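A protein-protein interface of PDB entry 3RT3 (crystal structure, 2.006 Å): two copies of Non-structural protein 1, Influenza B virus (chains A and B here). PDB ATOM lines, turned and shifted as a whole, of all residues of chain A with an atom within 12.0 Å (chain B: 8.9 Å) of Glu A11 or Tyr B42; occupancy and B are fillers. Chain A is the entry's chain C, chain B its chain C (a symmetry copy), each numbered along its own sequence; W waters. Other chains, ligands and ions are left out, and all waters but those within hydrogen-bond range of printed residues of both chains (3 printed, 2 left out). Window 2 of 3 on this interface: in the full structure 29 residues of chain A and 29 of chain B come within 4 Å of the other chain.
Of the 16 printed residues of chain B, 7 touch a printed residue of chain A. Printed residues of chain B that touch a printed residue of chain A: Arg B38, Ala B39, Leu B40, Asp B41, Tyr B42, Gln B45 and Arg B47. Among the printed residues, 17 pairs touch across the chains. Among the printed residues, Asp or Glu carboxylates within 4 Å of a Lys or Arg side-chain nitrogen of the other chain: Glu A24 with Arg B47 (2.7 Å).
No position is printed for both chains.
Of the printed residues of chain B, Glu A11 touches Tyr B42 (3.7 Å). No residue of chain A comes within 4 Å of Pro B43. No residue of chain A comes within 4 Å of Gly B44. Of chain A, only Gln A9 and Ile A10 come within 4 Å of Gln B45. No residue of chain A comes within 4 Å of Asp B46. Printed residues of chain A within 4 Å of Arg B38: Ile A10 and Val A12. Of the printed residues of chain B, Thr A17 touches Asp B41 (3.9 Å). Of the printed residues of chain B, Gln A9 touches Gln B45 (3.7 Å). Of the printed residues of chain B, Thr A20 touches Ala B39 (2.8 Å), Leu B40 (3.2 Å) and Asp B41 (2.8 Å). Printed residues of chain B within 4 Å of Arg A58: Arg B47 (3.1 Å). The nearest residue of chain A that does not touch Tyr B42 is Gly A13 (5.4 Å). The nearest printed residue of chain B that does not touch Gln A9 is His B49 (4.6 Å).
CA of Gln A9 touches NE2 of Gln B45, at 3.7 Å. CG2 of Ile A10 touches CG of Arg B38, at 3.8 Å. Tyr B42 touches Ile A10 (CE2 to O, 3.3 Å). Tyr B42 touches Glu A11. Arg B38 touches Val A12. O of Leu B40 touches CG1 of Val A12, at 3.6 Å. Ala A16 touches Asp B41. OD2 of Asp B41 touches CA of Thr A17, 3.9 Å away. CB of Ala A19 touches O of Ala B39 (3.9 Å). Leu B40 touches Thr A20.
Water W1 lies within hydrogen-bond range of OD2 of Asp B41, O of Thr A17 and NH2 of Arg A58. Water W3 bridges the side-chain hydroxyl (OG1) of Thr A17 (2.8 Å) and the side-chain carboxylate (OD2) of Asp B41 (2.8 Å). Water W2 bridges the backbone carbonyl oxygen (O) of Glu A11 (3.0 Å) and the guanidinium group (NE) of Arg B38 (3.1 Å).
The backbone carbonyl oxygen (O) of Leu B40 lies close to the side-chain amide oxygen (OE1) of Gln B45, at 3.0 Å. The backbone carbonyl oxygen (O) of Ala A16 is in hydrogen-bond range of the side-chain hydroxyl (OG1) of Thr A20, at 2.8 Å. OE1 of Glu A24 lies within salt-bridge range of NH2 of Arg A58, at 2.7 Å. The backbone NH (N) of Gly B44 sits at hydrogen-bond distance from the side-chain carboxylate (OD1) of Asp B41 (2.7 Å).
The side-chain carboxylate (OE2) of Glu A24 lies within salt-bridge range of the guanidinium group (NE) of Arg B47 (2.7 Å). NH2 of Arg A58 sits close to NH2 of Arg B47 (3.1 Å). The backbone carbonyl oxygen of Ala B39 sits close to the backbone carbonyl oxygen of Ala A16 (3.3 Å). The backbone NH (N) of Val A12 sits at hydrogen-bond distance from the side-chain hydroxyl (OH) of Tyr B42 (3.2 Å). The backbone carbonyl oxygen of Ile A10 sits close to the side-chain amide oxygen of Gln B45 (2.9 Å). OG1 of Thr A20 sits at hydrogen-bond distance from O of Ala B39 (2.8 Å). The backbone NH of Asp B41 is in hydrogen-bond range of the side-chain hydroxyl of Thr A20.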
ATOM      1  N   GLN A   9     -21.203 -19.461   4.990  1.00  0.00           N
ATOM      2  CA  GLN A   9     -20.180 -18.502   4.556  1.00  0.00           C
ATOM      3  C   GLN A   9     -19.549 -18.934   3.243  1.00  0.00           C
ATOM      4  O   GLN A   9     -18.594 -19.709   3.235  1.00  0.00           O
ATOM      5  CB  GLN A   9     -19.078 -18.371   5.603  1.00  0.00           C
ATOM      6  CG  GLN A   9     -19.478 -17.665   6.886  1.00  0.00           C
ATOM      7  CD  GLN A   9     -18.273 -17.318   7.744  1.00  0.00           C
ATOM      8  OE1 GLN A   9     -17.272 -16.798   7.248  1.00  0.00           O
ATOM      9  NE2 GLN A   9     -18.361 -17.613   9.036  1.00  0.00           N
ATOM     10  N   ILE A  10     -20.069 -18.423   2.131  1.00  0.00           N
ATOM     11  CA  ILE A  10     -19.628 -18.875   0.817  1.00  0.00           C
ATOM     12  C   ILE A  10     -18.713 -17.837   0.189  1.00  0.00           C
ATOM     13  O   ILE A  10     -19.080 -16.675   0.075  1.00  0.00           O
ATOM     14  CB  ILE A  10     -20.817 -19.122  -0.146  1.00  0.00           C
ATOM     15  CG1 ILE A  10     -21.635 -20.343   0.277  1.00  0.00           C
ATOM     16  CG2 ILE A  10     -20.304 -19.340  -1.564  1.00  0.00           C
ATOM     17  CD1 ILE A  10     -22.089 -20.341   1.710  1.00  0.00           C
ATOM     18  N   GLU A  11     -17.518 -18.262  -0.212  1.00  0.00           N
ATOM     19  CA  GLU A  11     -16.568 -17.374  -0.861  1.00  0.00           C
ATOM     20  C   GLU A  11     -17.072 -16.978  -2.250  1.00  0.00           C
ATOM     21  O   GLU A  11     -17.363 -17.832  -3.078  1.00  0.00           O
ATOM     22  CB  GLU A  11     -15.199 -18.056  -0.966  1.00  0.00           C
ATOM     23  CG  GLU A  11     -14.152 -17.254  -1.721  1.00  0.00           C
ATOM     24  CD  GLU A  11     -12.809 -17.982  -1.754  1.00  0.00           C
ATOM     25  OE1 GLU A  11     -11.852 -17.447  -2.351  1.00  0.00           O
ATOM     26  OE2 GLU A  11     -12.725 -19.096  -1.178  1.00  0.00           O
ATOM     27  N   VAL A  12     -17.177 -15.677  -2.499  1.00  0.00           N
ATOM     28  CA  VAL A  12     -17.625 -15.176  -3.795  1.00  0.00           C
ATOM     29  C   VAL A  12     -16.684 -14.055  -4.236  1.00  0.00           C
ATOM     30  O   VAL A  12     -15.964 -13.473  -3.414  1.00  0.00           O
ATOM     31  CB  VAL A  12     -19.048 -14.604  -3.733  1.00  0.00           C
ATOM     32  CG1 VAL A  12     -20.053 -15.682  -3.373  1.00  0.00           C
ATOM     33  CG2 VAL A  12     -19.108 -13.473  -2.719  1.00  0.00           C
ATOM     34  N   GLY A  13     -16.699 -13.748  -5.529  1.00  0.00           N
ATOM     35  CA  GLY A  13     -15.823 -12.729  -6.072  1.00  0.00           C
ATOM     36  C   GLY A  13     -16.565 -11.430  -6.258  1.00  0.00           C
ATOM     37  O   GLY A  13     -17.761 -11.349  -5.946  1.00  0.00           O
ATOM     38  N   PRO A  14     -15.857 -10.397  -6.748  1.00  0.00           N
ATOM     39  CA  PRO A  14     -16.524  -9.144  -7.110  1.00  0.00           C
ATOM     40  C   PRO A  14     -17.570  -9.447  -8.182  1.00  0.00           C
ATOM     41  O   PRO A  14     -17.441 -10.402  -8.941  1.00  0.00           O
ATOM     42  CB  PRO A  14     -15.387  -8.285  -7.702  1.00  0.00           C
ATOM     43  CG  PRO A  14     -14.112  -8.932  -7.259  1.00  0.00           C
ATOM     44  CD  PRO A  14     -14.429 -10.402  -7.112  1.00  0.00           C
ATOM     45  N   GLY A  15     -18.617  -8.655  -8.256  1.00  0.00           N
ATOM     46  CA  GLY A  15     -19.600  -8.942  -9.276  1.00  0.00           C
ATOM     47  C   GLY A  15     -20.584 -10.003  -8.835  1.00  0.00           C
ATOM     48  O   GLY A  15     -21.527 -10.311  -9.562  1.00  0.00           O
ATOM     49  N   ALA A  16     -20.354 -10.589  -7.661  1.00  0.00           N
ATOM     50  CA  ALA A  16     -21.473 -11.114  -6.909  1.00  0.00           C
ATOM     51  C   ALA A  16     -22.192  -9.855  -6.449  1.00  0.00           C
ATOM     52  O   ALA A  16     -23.377  -9.881  -6.134  1.00  0.00           O
ATOM     53  CB  ALA A  16     -21.026 -11.970  -5.724  1.00  0.00           C
ATOM     54  N   THR A  17     -21.478  -8.724  -6.444  1.00  0.00           N
ATOM     55  CA  THR A  17     -22.120  -7.473  -6.079  1.00  0.00           C
ATOM     56  C   THR A  17     -23.175  -7.107  -7.126  1.00  0.00           C
ATOM     57  O   THR A  17     -24.338  -6.894  -6.807  1.00  0.00           O
ATOM     58  CB  THR A  17     -21.103  -6.330  -5.927  1.00  0.00           C
ATOM     59  OG1 THR A  17     -20.201  -6.649  -4.859  1.00  0.00           O
ATOM     60  CG2 THR A  17     -21.830  -5.031  -5.599  1.00  0.00           C
ATOM     61  N   ASN A  18     -22.761  -7.068  -8.387  1.00  0.00           N
ATOM     62  CA  ASN A  18     -23.688  -6.805  -9.459  1.00  0.00           C
ATOM     63  C   ASN A  18     -24.795  -7.853  -9.495  1.00  0.00           C
ATOM     64  O   ASN A  18     -25.972  -7.505  -9.556  1.00  0.00           O
ATOM     65  CB  ASN A  18     -22.962  -6.748 -10.794  1.00  0.00           C
ATOM     66  CG  ASN A  18     -23.875  -6.328 -11.927  1.00  0.00           C
ATOM     67  OD1 ASN A  18     -24.378  -5.201 -11.958  1.00  0.00           O
ATOM     68  ND2 ASN A  18     -24.088  -7.229 -12.871  1.00  0.00           N
ATOM     69  N   ALA A  19     -24.420  -9.132  -9.442  1.00  0.00           N
ATOM     70  CA  ALA A  19     -25.405 -10.207  -9.550  1.00  0.00           C
ATOM     71  C   ALA A  19     -26.429 -10.148  -8.427  1.00  0.00           C
ATOM     72  O   ALA A  19     -27.606 -10.408  -8.646  1.00  0.00           O
ATOM     73  CB  ALA A  19     -24.727 -11.559  -9.590  1.00  0.00           C
ATOM     74  N   THR A  20     -25.987  -9.797  -7.224  1.00  0.00           N
ATOM     75  CA  THR A  20     -26.900  -9.752  -6.094  1.00  0.00           C
ATOM     76  C   THR A  20     -27.822  -8.545  -6.215  1.00  0.00           C
ATOM     77  O   THR A  20     -28.988  -8.610  -5.853  1.00  0.00           O
ATOM     78  CB  THR A  20     -26.150  -9.760  -4.759  1.00  0.00           C
ATOM     79  OG1 THR A  20     -25.438 -11.000  -4.630  1.00  0.00           O
ATOM     80  CG2 THR A  20     -27.129  -9.632  -3.588  1.00  0.00           C
ATOM     81  N   ILE A  21     -27.310  -7.448  -6.760  1.00  0.00           N
ATOM     82  CA  ILE A  21     -28.176  -6.314  -7.032  1.00  0.00           C
ATOM     83  C   ILE A  21     -29.278  -6.742  -8.005  1.00  0.00           C
ATOM     84  O   ILE A  21     -30.467  -6.474  -7.788  1.00  0.00           O
ATOM     85  CB  ILE A  21     -27.379  -5.106  -7.595  1.00  0.00           C
ATOM     86  CG1 ILE A  21     -26.479  -4.498  -6.514  1.00  0.00           C
ATOM     87  CG2 ILE A  21     -28.314  -4.049  -8.134  1.00  0.00           C
ATOM     88  CD1 ILE A  21     -25.805  -3.160  -6.945  1.00  0.00           C
ATOM     89  N   PHE A  23     -30.302  -9.875  -8.788  1.00  0.00           N
ATOM     90  CA  PHE A  23     -31.136 -10.868  -8.116  1.00  0.00           C
ATOM     91  C   PHE A  23     -32.188 -10.204  -7.216  1.00  0.00           C
ATOM     92  O   PHE A  23     -33.352 -10.572  -7.230  1.00  0.00           O
ATOM     93  CB  PHE A  23     -30.275 -11.818  -7.285  1.00  0.00           C
ATOM     94  CG  PHE A  23     -31.076 -12.763  -6.420  1.00  0.00           C
ATOM     95  CD1 PHE A  23     -31.781 -13.826  -6.990  1.00  0.00           C
ATOM     96  CD2 PHE A  23     -31.123 -12.592  -5.040  1.00  0.00           C
ATOM     97  CE1 PHE A  23     -32.531 -14.716  -6.191  1.00  0.00           C
ATOM     98  CE2 PHE A  23     -31.859 -13.473  -4.240  1.00  0.00           C
ATOM     99  CZ  PHE A  23     -32.561 -14.533  -4.825  1.00  0.00           C
ATOM    100  N   GLU A  24     -31.777  -9.218  -6.431  1.00  0.00           N
ATOM    101  CA  GLU A  24     -32.704  -8.634  -5.474  1.00  0.00           C
ATOM    102  C   GLU A  24     -33.687  -7.657  -6.122  1.00  0.00           C
ATOM    103  O   GLU A  24     -34.772  -7.408  -5.587  1.00  0.00           O
ATOM    104  CB  GLU A  24     -31.962  -8.035  -4.282  1.00  0.00           C
ATOM    105  CG  GLU A  24     -31.382  -9.095  -3.366  1.00  0.00           C
ATOM    106  CD  GLU A  24     -30.677  -8.507  -2.168  1.00  0.00           C
ATOM    107  OE1 GLU A  24     -29.828  -7.628  -2.370  1.00  0.00           O
ATOM    108  OE2 GLU A  24     -30.961  -8.922  -1.029  1.00  0.00           O
ATOM    109  N   ARG A  58     -28.297   1.611  -3.772  1.00  0.00           N
ATOM    110  CA  ARG A  58     -27.258   0.642  -4.114  1.00  0.00           C
ATOM    111  C   ARG A  58     -26.963   0.658  -5.614  1.00  0.00           C
ATOM    112  O   ARG A  58     -25.801   0.646  -6.029  1.00  0.00           O
ATOM    113  CB  ARG A  58     -27.645  -0.766  -3.656  1.00  0.00           C
ATOM    114  CG  ARG A  58     -27.347  -1.058  -2.188  1.00  0.00           C
ATOM    115  CD  ARG A  58     -28.103  -2.297  -1.700  1.00  0.00           C
ATOM    116  NE  ARG A  58     -27.713  -3.519  -2.403  1.00  0.00           N
ATOM    117  CZ  ARG A  58     -28.416  -4.648  -2.377  1.00  0.00           C
ATOM    118  NH1 ARG A  58     -29.562  -4.710  -1.698  1.00  0.00           N
ATOM    119  NH2 ARG A  58     -27.981  -5.715  -3.040  1.00  0.00           N
ATOM    120  N   SER B  35     -27.422 -18.608  -3.734  1.00  0.00           N
ATOM    121  CA  SER B  35     -26.156 -18.722  -3.012  1.00  0.00           C
ATOM    122  C   SER B  35     -25.339 -19.913  -3.517  1.00  0.00           C
ATOM    123  O   SER B  35     -24.113 -19.888  -3.492  1.00  0.00           O
ATOM    124  CB  SER B  35     -26.420 -18.888  -1.516  1.00  0.00           C
ATOM    125  OG  SER B  35     -25.345 -18.338  -0.770  1.00  0.00           O
ATOM    126  N   TRP B  36     -26.023 -20.959  -3.973  1.00  0.00           N
ATOM    127  CA  TRP B  36     -25.333 -22.137  -4.514  1.00  0.00           C
ATOM    128  C   TRP B  36     -24.514 -21.810  -5.776  1.00  0.00           C
ATOM    129  O   TRP B  36     -23.588 -22.537  -6.131  1.00  0.00           O
ATOM    130  CB  TRP B  36     -26.348 -23.234  -4.855  1.00  0.00           C
ATOM    131  CG  TRP B  36     -27.171 -23.731  -3.688  1.00  0.00           C
ATOM    132  CD1 TRP B  36     -26.898 -23.590  -2.347  1.00  0.00           C
ATOM    133  CD2 TRP B  36     -28.402 -24.462  -3.775  1.00  0.00           C
ATOM    134  NE1 TRP B  36     -27.896 -24.188  -1.604  1.00  0.00           N
ATOM    135  CE2 TRP B  36     -28.826 -24.730  -2.456  1.00  0.00           C
ATOM    136  CE3 TRP B  36     -29.184 -24.915  -4.843  1.00  0.00           C
ATOM    137  CZ2 TRP B  36     -29.993 -25.438  -2.180  1.00  0.00           C
ATOM    138  CZ3 TRP B  36     -30.338 -25.624  -4.568  1.00  0.00           C
ATOM    139  CH2 TRP B  36     -30.736 -25.869  -3.246  1.00  0.00           C
ATOM    140  N   GLN B  37     -24.884 -20.735  -6.463  1.00  0.00           N
ATOM    141  CA  GLN B  37     -24.206 -20.333  -7.698  1.00  0.00           C
ATOM    142  C   GLN B  37     -22.968 -19.495  -7.406  1.00  0.00           C
ATOM    143  O   GLN B  37     -22.265 -19.094  -8.318  1.00  0.00           O
ATOM    144  CB  GLN B  37     -25.147 -19.516  -8.569  1.00  0.00           C
ATOM    145  CG  GLN B  37     -26.555 -20.098  -8.682  1.00  0.00           C
ATOM    146  CD  GLN B  37     -26.542 -21.599  -8.918  1.00  0.00           C
ATOM    147  OE1 GLN B  37     -25.858 -22.103  -9.826  1.00  0.00           O
ATOM    148  NE2 GLN B  37     -27.293 -22.327  -8.090  1.00  0.00           N
ATOM    149  N   ARG B  38     -22.744 -19.226  -6.122  1.00  0.00           N
ATOM    150  CA  ARG B  38     -21.679 -18.361  -5.656  1.00  0.00           C
ATOM    151  C   ARG B  38     -21.875 -16.943  -6.152  1.00  0.00           C
ATOM    152  O   ARG B  38     -20.913 -16.251  -6.397  1.00  0.00           O
ATOM    153  CB  ARG B  38     -20.300 -18.900  -6.051  1.00  0.00           C
ATOM    154  CG  ARG B  38     -19.862 -20.099  -5.230  1.00  0.00           C
ATOM    155  CD  ARG B  38     -18.752 -20.861  -5.930  1.00  0.00           C
ATOM    156  NE  ARG B  38     -18.546 -22.169  -5.316  1.00  0.00           N
ATOM    157  CZ  ARG B  38     -17.734 -23.105  -5.797  1.00  0.00           C
ATOM    158  NH1 ARG B  38     -17.043 -22.881  -6.907  1.00  0.00           N
ATOM    159  NH2 ARG B  38     -17.616 -24.267  -5.165  1.00  0.00           N
ATOM    160  N   ALA B  39     -23.132 -16.513  -6.242  1.00  0.00           N
ATOM    161  CA  ALA B  39     -23.479 -15.207  -6.782  1.00  0.00           C
ATOM    162  C   ALA B  39     -24.009 -14.236  -5.725  1.00  0.00           C
ATOM    163  O   ALA B  39     -24.184 -13.046  -6.000  1.00  0.00           O
ATOM    164  CB  ALA B  39     -24.506 -15.372  -7.898  1.00  0.00           C
ATOM    165  N   LEU B  40     -24.289 -14.743  -4.523  1.00  0.00           N
ATOM    166  CA  LEU B  40     -24.832 -13.895  -3.470  1.00  0.00           C
ATOM    167  C   LEU B  40     -23.700 -13.259  -2.656  1.00  0.00           C
ATOM    168  O   LEU B  40     -22.924 -13.974  -2.012  1.00  0.00           O
ATOM    169  CB  LEU B  40     -25.732 -14.717  -2.550  1.00  0.00           C
ATOM    170  CG  LEU B  40     -26.512 -13.973  -1.476  1.00  0.00           C
ATOM    171  CD1 LEU B  40     -27.502 -12.990  -2.134  1.00  0.00           C
ATOM    172  CD2 LEU B  40     -27.248 -14.983  -0.581  1.00  0.00           C
ATOM    173  N   ASP B  41     -23.602 -11.928  -2.672  1.00  0.00           N
ATOM    174  CA  ASP B  41     -22.486 -11.241  -1.988  1.00  0.00           C
ATOM    175  C   ASP B  41     -22.604 -11.363  -0.470  1.00  0.00           C
ATOM    176  O   ASP B  41     -23.603 -11.874   0.035  1.00  0.00           O
ATOM    177  CB  ASP B  41     -22.369  -9.770  -2.421  1.00  0.00           C
ATOM    178  CG  ASP B  41     -23.596  -8.940  -2.041  1.00  0.00           C
ATOM    179  OD1 ASP B  41     -24.453  -9.449  -1.293  1.00  0.00           O
ATOM    180  OD2 ASP B  41     -23.689  -7.764  -2.475  1.00  0.00           O
ATOM    181  N   TYR B  42     -21.601 -10.894   0.268  1.00  0.00           N
ATOM    182  CA  TYR B  42     -21.592 -11.118   1.715  1.00  0.00           C
ATOM    183  C   TYR B  42     -22.729 -10.428   2.464  1.00  0.00           C
ATOM    184  O   TYR B  42     -23.303 -11.000   3.388  1.00  0.00           O
ATOM    185  CB  TYR B  42     -20.243 -10.764   2.315  1.00  0.00           C
ATOM    186  CG  TYR B  42     -19.135 -11.568   1.680  1.00  0.00           C
ATOM    187  CD1 TYR B  42     -18.113 -10.949   0.972  1.00  0.00           C
ATOM    188  CD2 TYR B  42     -19.141 -12.954   1.747  1.00  0.00           C
ATOM    189  CE1 TYR B  42     -17.105 -11.688   0.372  1.00  0.00           C
ATOM    190  CE2 TYR B  42     -18.148 -13.698   1.150  1.00  0.00           C
ATOM    191  CZ  TYR B  42     -17.129 -13.060   0.466  1.00  0.00           C
ATOM    192  OH  TYR B  42     -16.151 -13.807  -0.132  1.00  0.00           O
ATOM    193  N   PRO B  43     -23.057  -9.192   2.078  1.00  0.00           N
ATOM    194  CA  PRO B  43     -24.241  -8.588   2.691  1.00  0.00           C
ATOM    195  C   PRO B  43     -25.472  -9.435   2.381  1.00  0.00           C
ATOM    196  O   PRO B  43     -26.346  -9.578   3.236  1.00  0.00           O
ATOM    197  CB  PRO B  43     -24.331  -7.236   1.991  1.00  0.00           C
ATOM    198  CG  PRO B  43     -22.902  -6.913   1.643  1.00  0.00           C
ATOM    199  CD  PRO B  43     -22.323  -8.237   1.227  1.00  0.00           C
ATOM    200  N   GLY B  44     -25.527  -9.996   1.175  1.00  0.00           N
ATOM    201  CA  GLY B  44     -26.666 -10.807   0.760  1.00  0.00           C
ATOM    202  C   GLY B  44     -26.815 -12.086   1.565  1.00  0.00           C
ATOM    203  O   GLY B  44     -27.925 -12.504   1.918  1.00  0.00           O
ATOM    204  N   GLN B  45     -25.686 -12.712   1.857  1.00  0.00           N
ATOM    205  CA  GLN B  45     -25.664 -13.917   2.667  1.00  0.00           C
ATOM    206  C   GLN B  45     -26.145 -13.602   4.077  1.00  0.00           C
ATOM    207  O   GLN B  45     -26.836 -14.412   4.700  1.00  0.00           O
ATOM    208  CB  GLN B  45     -24.252 -14.495   2.694  1.00  0.00           C
ATOM    209  CG  GLN B  45     -23.749 -14.888   1.318  1.00  0.00           C
ATOM    210  CD  GLN B  45     -22.328 -15.434   1.328  1.00  0.00           C
ATOM    211  OE1 GLN B  45     -21.555 -15.227   0.380  1.00  0.00           O
ATOM    212  NE2 GLN B  45     -21.979 -16.148   2.392  1.00  0.00           N
ATOM    213  N   ASP B  46     -25.755 -12.430   4.575  1.00  0.00           N
ATOM    214  CA  ASP B  46     -26.254 -11.927   5.855  1.00  0.00           C
ATOM    215  C   ASP B  46     -27.767 -11.718   5.813  1.00  0.00           C
ATOM    216  O   ASP B  46     -28.481 -12.096   6.738  1.00  0.00           O
ATOM    217  CB  ASP B  46     -25.558 -10.616   6.232  1.00  0.00           C
ATOM    218  CG  ASP B  46     -24.225 -10.841   6.938  1.00  0.00           C
ATOM    219  OD1 ASP B  46     -23.250 -11.263   6.274  1.00  0.00           O
ATOM    220  OD2 ASP B  46     -24.151 -10.584   8.161  1.00  0.00           O
ATOM    221  N   ARG B  47     -28.263 -11.115   4.737  1.00  0.00           N
ATOM    222  CA  ARG B  47     -29.710 -10.999   4.588  1.00  0.00           C
ATOM    223  C   ARG B  47     -30.381 -12.377   4.614  1.00  0.00           C
ATOM    224  O   ARG B  47     -31.420 -12.554   5.244  1.00  0.00           O
ATOM    225  CB  ARG B  47     -30.093 -10.200   3.332  1.00  0.00           C
ATOM    226  CG  ARG B  47     -29.833  -8.687   3.466  1.00  0.00           C
ATOM    227  CD  ARG B  47     -30.508  -7.861   2.364  1.00  0.00           C
ATOM    228  NE  ARG B  47     -29.772  -7.831   1.096  1.00  0.00           N
ATOM    229  CZ  ARG B  47     -28.623  -7.190   0.904  1.00  0.00           C
ATOM    230  NH1 ARG B  47     -28.040  -6.550   1.910  1.00  0.00           N
ATOM    231  NH2 ARG B  47     -28.042  -7.209  -0.288  1.00  0.00           N
ATOM    232  N   LEU B  48     -29.779 -13.360   3.954  1.00  0.00           N
ATOM    233  CA  LEU B  48     -30.378 -14.696   3.907  1.00  0.00           C
ATOM    234  C   LEU B  48     -30.494 -15.304   5.308  1.00  0.00           C
ATOM    235  O   LEU B  48     -31.554 -15.800   5.706  1.00  0.00           O
ATOM    236  CB  LEU B  48     -29.583 -15.617   2.957  1.00  0.00           C
ATOM    237  CG  LEU B  48     -29.844 -17.135   2.907  1.00  0.00           C
ATOM    238  CD1 LEU B  48     -29.010 -17.780   1.783  1.00  0.00           C
ATOM    239  CD2 LEU B  48     -29.495 -17.790   4.220  1.00  0.00           C
ATOM    240  N   HIS B  49     -29.397 -15.261   6.049  1.00  0.00           N
ATOM    241  CA  HIS B  49     -29.362 -15.864   7.368  1.00  0.00           C
ATOM    242  C   HIS B  49     -30.374 -15.215   8.302  1.00  0.00           C
ATOM    243  O   HIS B  49     -30.993 -15.901   9.118  1.00  0.00           O
ATOM    244  CB  HIS B  49     -27.950 -15.798   7.953  1.00  0.00           C
ATOM    245  CG  HIS B  49     -26.937 -16.551   7.150  1.00  0.00           C
ATOM    246  ND1 HIS B  49     -27.248 -17.693   6.446  1.00  0.00           N
ATOM    247  CD2 HIS B  49     -25.622 -16.316   6.924  1.00  0.00           C
ATOM    248  CE1 HIS B  49     -26.167 -18.136   5.827  1.00  0.00           C
ATOM    249  NE2 HIS B  49     -25.167 -17.318   6.101  1.00  0.00           N
ATOM    250  N   ARG B  50     -30.558 -13.906   8.160  1.00  0.00           N
ATOM    251  CA  ARG B  50     -31.478 -13.181   9.012  1.00  0.00           C
ATOM    252  C   ARG B  50     -32.915 -13.498   8.650  1.00  0.00           C
ATOM    253  O   ARG B  50     -33.779 -13.574   9.520  1.00  0.00           O
ATOM    254  CB  ARG B  50     -31.211 -11.681   8.921  1.00  0.00           C
ATOM    255  CG  ARG B  50     -29.892 -11.275   9.574  1.00  0.00           C
ATOM    256  CD  ARG B  50     -29.580  -9.796   9.390  1.00  0.00           C
ATOM    257  NE  ARG B  50     -28.475  -9.372  10.252  1.00  0.00           N
ATOM    258  CZ  ARG B  50     -27.187  -9.578   9.982  1.00  0.00           C
ATOM    259  NH1 ARG B  50     -26.827 -10.208   8.869  1.00  0.00           N
ATOM    260  NH2 ARG B  50     -26.253  -9.154  10.828  1.00  0.00           N
HETATM  261  O   HOH W   1     -25.064  -6.132  -4.142  1.00  0.00           O
HETATM  262  O   HOH W   2     -17.311 -20.847  -2.765  1.00  0.00           O
HETATM  263  O   HOH W   3     -21.237  -6.403  -2.322  1.00  0.00           O
